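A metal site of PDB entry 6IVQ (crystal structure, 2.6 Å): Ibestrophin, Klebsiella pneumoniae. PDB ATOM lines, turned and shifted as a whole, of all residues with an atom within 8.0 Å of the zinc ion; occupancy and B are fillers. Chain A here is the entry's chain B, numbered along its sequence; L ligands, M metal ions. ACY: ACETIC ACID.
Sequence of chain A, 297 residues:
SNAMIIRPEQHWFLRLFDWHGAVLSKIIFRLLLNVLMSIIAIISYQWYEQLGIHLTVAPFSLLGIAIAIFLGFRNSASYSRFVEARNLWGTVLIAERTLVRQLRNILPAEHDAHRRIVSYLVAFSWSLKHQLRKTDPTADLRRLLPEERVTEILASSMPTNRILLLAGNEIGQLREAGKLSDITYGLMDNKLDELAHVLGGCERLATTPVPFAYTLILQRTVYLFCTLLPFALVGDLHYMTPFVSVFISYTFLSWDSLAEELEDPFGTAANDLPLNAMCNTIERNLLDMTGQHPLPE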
ATOM      1  N   VAL A 100     -14.912  24.716  11.444  1.00  0.00           N
ATOM      2  CA  VAL A 100     -16.129  24.411  10.720  1.00  0.00           C
ATOM      3  C   VAL A 100     -15.990  24.824   9.252  1.00  0.00           C
ATOM      4  O   VAL A 100     -16.403  24.084   8.358  1.00  0.00           O
ATOM      5  CB  VAL A 100     -17.352  25.066  11.406  1.00  0.00           C
ATOM      6  CG1 VAL A 100     -18.570  25.132  10.506  1.00  0.00           C
ATOM      7  CG2 VAL A 100     -17.670  24.356  12.697  1.00  0.00           C
ATOM      8  N   LEU A 103     -13.846  22.318   7.392  1.00  0.00           N
ATOM      9  CA  LEU A 103     -14.623  21.109   7.155  1.00  0.00           C
ATOM     10  C   LEU A 103     -15.612  21.329   6.011  1.00  0.00           C
ATOM     11  O   LEU A 103     -15.733  20.461   5.154  1.00  0.00           O
ATOM     12  CB  LEU A 103     -15.345  20.690   8.440  1.00  0.00           C
ATOM     13  CG  LEU A 103     -14.514  19.942   9.467  1.00  0.00           C
ATOM     14  CD1 LEU A 103     -15.278  19.867  10.779  1.00  0.00           C
ATOM     15  CD2 LEU A 103     -14.143  18.541   8.981  1.00  0.00           C
ATOM     16  N   ARG A 104     -16.305  22.477   5.997  1.00  0.00           N
ATOM     17  CA  ARG A 104     -17.224  22.809   4.919  1.00  0.00           C
ATOM     18  C   ARG A 104     -16.460  22.988   3.615  1.00  0.00           C
ATOM     19  O   ARG A 104     -16.961  22.601   2.561  1.00  0.00           O
ATOM     20  CB  ARG A 104     -18.106  24.028   5.240  1.00  0.00           C
ATOM     21  CG  ARG A 104     -19.117  23.750   6.345  1.00  0.00           C
ATOM     22  CD  ARG A 104     -19.884  24.929   6.893  1.00  0.00           C
ATOM     23  NE  ARG A 104     -21.013  24.525   7.753  1.00  0.00           N
ATOM     24  CZ  ARG A 104     -21.711  25.357   8.548  1.00  0.00           C
ATOM     25  NH1 ARG A 104     -22.730  24.894   9.249  1.00  0.00           N
ATOM     26  NH2 ARG A 104     -21.370  26.632   8.656  1.00  0.00           N
ATOM     27  N   LEU A 107     -14.391  19.141   2.896  1.00  0.00           N
ATOM     28  CA  LEU A 107     -15.256  17.984   2.873  1.00  0.00           C
ATOM     29  C   LEU A 107     -16.699  18.488   2.794  1.00  0.00           C
ATOM     30  O   LEU A 107     -17.500  18.244   3.691  1.00  0.00           O
ATOM     31  CB  LEU A 107     -15.012  17.180   4.158  1.00  0.00           C
ATOM     32  CG  LEU A 107     -13.640  16.513   4.257  1.00  0.00           C
ATOM     33  CD1 LEU A 107     -13.459  15.803   5.602  1.00  0.00           C
ATOM     34  CD2 LEU A 107     -13.439  15.549   3.103  1.00  0.00           C
ATOM     35  N   PRO A 108     -17.057  19.224   1.711  1.00  0.00           N
ATOM     36  CA  PRO A 108     -18.342  19.908   1.647  1.00  0.00           C
ATOM     37  C   PRO A 108     -19.581  19.040   1.851  1.00  0.00           C
ATOM     38  O   PRO A 108     -20.629  19.539   2.275  1.00  0.00           O
ATOM     39  CB  PRO A 108     -18.335  20.573   0.262  1.00  0.00           C
ATOM     40  CG  PRO A 108     -17.249  19.869  -0.516  1.00  0.00           C
ATOM     41  CD  PRO A 108     -16.229  19.460   0.516  1.00  0.00           C
ATOM     42  N   ALA A 109     -19.452  17.736   1.571  1.00  0.00           N
ATOM     43  CA  ALA A 109     -20.591  16.835   1.487  1.00  0.00           C
ATOM     44  C   ALA A 109     -20.751  16.032   2.779  1.00  0.00           C
ATOM     45  O   ALA A 109     -21.795  15.427   3.005  1.00  0.00           O
ATOM     46  CB  ALA A 109     -20.429  15.935   0.291  1.00  0.00           C
ATOM     47  N   GLU A 110     -19.735  16.044   3.644  1.00  0.00           N
ATOM     48  CA  GLU A 110     -19.665  15.201   4.836  1.00  0.00           C
ATOM     49  C   GLU A 110     -20.449  15.803   6.007  1.00  0.00           C
ATOM     50  O   GLU A 110     -19.887  15.986   7.096  1.00  0.00           O
ATOM     51  CB  GLU A 110     -18.191  15.053   5.208  1.00  0.00           C
ATOM     52  CG  GLU A 110     -17.390  14.273   4.179  1.00  0.00           C
ATOM     53  CD  GLU A 110     -17.680  12.777   4.075  1.00  0.00           C
ATOM     54  OE1 GLU A 110     -18.109  12.173   5.097  1.00  0.00           O
ATOM     55  OE2 GLU A 110     -17.487  12.226   2.972  1.00  0.00           O
ATOM     56  N   HIS A 111     -21.754  16.020   5.817  1.00  0.00           N
ATOM     57  CA  HIS A 111     -22.616  16.641   6.812  1.00  0.00           C
ATOM     58  C   HIS A 111     -22.711  15.849   8.132  1.00  0.00           C
ATOM     59  O   HIS A 111     -22.907  16.452   9.192  1.00  0.00           O
ATOM     60  CB  HIS A 111     -23.992  16.964   6.219  1.00  0.00           C
ATOM     61  CG  HIS A 111     -23.925  17.744   4.965  1.00  0.00           C
ATOM     62  ND1 HIS A 111     -23.391  19.027   4.906  1.00  0.00           N
ATOM     63  CD2 HIS A 111     -24.307  17.439   3.701  1.00  0.00           C
ATOM     64  CE1 HIS A 111     -23.460  19.477   3.668  1.00  0.00           C
ATOM     65  NE2 HIS A 111     -24.014  18.517   2.903  1.00  0.00           N
ATOM     66  N   ASP A 112     -22.573  14.520   8.105  1.00  0.00           N
ATOM     67  CA  ASP A 112     -22.689  13.791   9.359  1.00  0.00           C
ATOM     68  C   ASP A 112     -21.519  14.144  10.277  1.00  0.00           C
ATOM     69  O   ASP A 112     -21.692  14.293  11.484  1.00  0.00           O
ATOM     70  CB  ASP A 112     -22.963  12.291   9.156  1.00  0.00           C
ATOM     71  CG  ASP A 112     -24.343  12.004   8.566  1.00  0.00           C
ATOM     72  OD1 ASP A 112     -25.343  12.587   9.055  1.00  0.00           O
ATOM     73  OD2 ASP A 112     -24.404  11.222   7.595  1.00  0.00           O
ATOM     74  N   ALA A 113     -20.333  14.303   9.664  1.00  0.00           N
ATOM     75  CA  ALA A 113     -19.137  14.675  10.394  1.00  0.00           C
ATOM     76  C   ALA A 113     -19.260  16.138  10.824  1.00  0.00           C
ATOM     77  O   ALA A 113     -19.027  16.455  11.989  1.00  0.00           O
ATOM     78  CB  ALA A 113     -17.913  14.398   9.553  1.00  0.00           C
ATOM     79  N   HIS A 114     -19.705  16.995   9.895  1.00  0.00           N
ATOM     80  CA  HIS A 114     -19.977  18.391  10.202  1.00  0.00           C
ATOM     81  C   HIS A 114     -20.781  18.492  11.490  1.00  0.00           C
ATOM     82  O   HIS A 114     -20.404  19.251  12.396  1.00  0.00           O
ATOM     83  CB  HIS A 114     -20.707  19.091   9.051  1.00  0.00           C
ATOM     84  CG  HIS A 114     -19.931  19.150   7.776  1.00  0.00           C
ATOM     85  ND1 HIS A 114     -20.540  19.480   6.576  1.00  0.00           N
ATOM     86  CD2 HIS A 114     -18.637  18.888   7.503  1.00  0.00           C
ATOM     87  CE1 HIS A 114     -19.634  19.430   5.606  1.00  0.00           C
ATOM     88  NE2 HIS A 114     -18.445  19.073   6.162  1.00  0.00           N
ATOM     89  N   ARG A 115     -21.880  17.715  11.564  1.00  0.00           N
ATOM     90  CA  ARG A 115     -22.826  17.765  12.668  1.00  0.00           C
ATOM     91  C   ARG A 115     -22.176  17.208  13.934  1.00  0.00           C
ATOM     92  O   ARG A 115     -22.331  17.764  15.018  1.00  0.00           O
ATOM     93  CB  ARG A 115     -24.116  17.049  12.296  1.00  0.00           C
ATOM     94  CG  ARG A 115     -25.206  17.089  13.358  1.00  0.00           C
ATOM     95  CD  ARG A 115     -26.408  16.219  13.023  1.00  0.00           C
ATOM     96  NE  ARG A 115     -26.042  14.876  12.558  1.00  0.00           N
ATOM     97  CZ  ARG A 115     -25.551  13.890  13.320  1.00  0.00           C
ATOM     98  NH1 ARG A 115     -25.498  14.024  14.640  1.00  0.00           N
ATOM     99  NH2 ARG A 115     -25.099  12.787  12.752  1.00  0.00           N
ATOM    100  N   VAL A 118     -19.375  19.721  15.153  1.00  0.00           N
ATOM    101  CA  VAL A 118     -19.953  20.953  15.657  1.00  0.00           C
ATOM    102  C   VAL A 118     -20.514  20.755  17.058  1.00  0.00           C
ATOM    103  O   VAL A 118     -20.503  21.676  17.876  1.00  0.00           O
ATOM    104  CB  VAL A 118     -20.990  21.544  14.691  1.00  0.00           C
ATOM    105  CG1 VAL A 118     -22.015  22.402  15.430  1.00  0.00           C
ATOM    106  CG2 VAL A 118     -20.286  22.349  13.600  1.00  0.00           C
ATOM    107  N   THR A 290     -29.796  25.599  10.923  1.00  0.00           N
ATOM    108  CA  THR A 290     -29.778  24.149  11.089  1.00  0.00           C
ATOM    109  C   THR A 290     -28.482  23.587  10.506  1.00  0.00           C
ATOM    110  O   THR A 290     -28.461  22.447  10.028  1.00  0.00           O
ATOM    111  CB  THR A 290     -31.076  23.466  10.611  1.00  0.00           C
ATOM    112  OG1 THR A 290     -31.144  23.554   9.187  1.00  0.00           O
ATOM    113  CG2 THR A 290     -32.339  24.033  11.208  1.00  0.00           C
ATOM    114  N   GLY A 291     -27.430  24.410  10.492  1.00  0.00           N
ATOM    115  CA  GLY A 291     -26.104  23.960  10.108  1.00  0.00           C
ATOM    116  C   GLY A 291     -25.924  23.829   8.602  1.00  0.00           C
ATOM    117  O   GLY A 291     -24.949  23.250   8.161  1.00  0.00           O
ATOM    118  N   GLN A 292     -26.841  24.426   7.849  1.00  0.00           N
ATOM    119  CA  GLN A 292     -26.801  24.346   6.362  1.00  0.00           C
ATOM    120  C   GLN A 292     -25.798  25.359   5.799  1.00  0.00           C
ATOM    121  O   GLN A 292     -25.705  26.442   6.335  1.00  0.00           O
ATOM    122  CB  GLN A 292     -28.200  24.599   5.815  1.00  0.00           C
ATOM    123  CG  GLN A 292     -29.183  23.520   6.186  1.00  0.00           C
ATOM    124  CD  GLN A 292     -30.524  23.738   5.537  1.00  0.00           C
ATOM    125  OE1 GLN A 292     -30.643  24.553   4.631  1.00  0.00           O
ATOM    126  NE2 GLN A 292     -31.523  23.018   5.992  1.00  0.00           N
ATOM    127  N   HIS A 293     -25.103  24.985   4.728  1.00  0.00           N
ATOM    128  CA  HIS A 293     -24.089  25.866   4.099  1.00  0.00           C
ATOM    129  C   HIS A 293     -24.154  25.764   2.580  1.00  0.00           C
ATOM    130  O   HIS A 293     -24.603  24.751   2.084  1.00  0.00           O
ATOM    131  CB  HIS A 293     -22.691  25.495   4.606  1.00  0.00           C
ATOM    132  CG  HIS A 293     -22.418  24.032   4.682  1.00  0.00           C
ATOM    133  ND1 HIS A 293     -21.540  23.403   3.828  1.00  0.00           N
ATOM    134  CD2 HIS A 293     -22.888  23.088   5.510  1.00  0.00           C
ATOM    135  CE1 HIS A 293     -21.511  22.126   4.135  1.00  0.00           C
ATOM    136  NE2 HIS A 293     -22.324  21.897   5.183  1.00  0.00           N
ATOM    137  N   PRO A 294     -23.757  26.808   1.826  1.00  0.00           N
ATOM    138  CA  PRO A 294     -23.725  26.771   0.379  1.00  0.00           C
ATOM    139  C   PRO A 294     -22.634  25.819  -0.151  1.00  0.00           C
ATOM    140  O   PRO A 294     -21.673  25.644   0.539  1.00  0.00           O
ATOM    141  CB  PRO A 294     -23.312  28.191  -0.003  1.00  0.00           C
ATOM    142  CG  PRO A 294     -23.710  29.019   1.171  1.00  0.00           C
ATOM    143  CD  PRO A 294     -23.421  28.115   2.345  1.00  0.00           C
ATOM    144  N   LEU A 295     -22.853  25.245  -1.341  1.00  0.00           N
ATOM    145  CA  LEU A 295     -21.917  24.303  -2.012  1.00  0.00           C
ATOM    146  C   LEU A 295     -21.603  23.131  -1.075  1.00  0.00           C
ATOM    147  O   LEU A 295     -22.543  22.378  -0.773  1.00  0.00           O
ATOM    148  CB  LEU A 295     -20.643  25.042  -2.443  1.00  0.00           C
ATOM    149  CG  LEU A 295     -19.575  24.207  -3.135  1.00  0.00           C
ATOM    150  CD1 LEU A 295     -19.057  24.879  -4.384  1.00  0.00           C
ATOM    151  CD2 LEU A 295     -18.430  23.888  -2.200  1.00  0.00           C
HETATM  152  C   ACY L   1     -23.420  21.030   8.990  1.00  0.00           C
HETATM  153  O   ACY L   1     -23.782  20.272   8.050  1.00  0.00           O
HETATM  154  OXT ACY L   1     -22.434  21.788   8.720  1.00  0.00           O
HETATM  155  CH3 ACY L   1     -24.144  21.034  10.379  1.00  0.00           C
HETATM  156 ZN    ZN M   1     -22.357  20.236   6.281  1.00  0.00          ZN
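A ring nitrogen (NE2) of His 114 is in hydrogen-bond range of the backbone carbonyl oxygen (O) of Leu 107 (2.8 Å).
NE2 of His 114 lies within hydrogen-bond range of O of Leu 103.
Of the 19 residues printed, 3 come within 4 Å of the zinc ion.
ND1 of His 114 is bound to the zinc ion (2.0 Å).
A ring nitrogen (NE2) of His 293 binds the zinc ion, at 2.0 Å.
A ring nitrogen (ND1) of His 111 is bound to the zinc ion, at 2.1 Å.
The zinc ion is bound by O of the ligand (2.3 Å).
The zinc ion has four donor atoms within binding distance.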
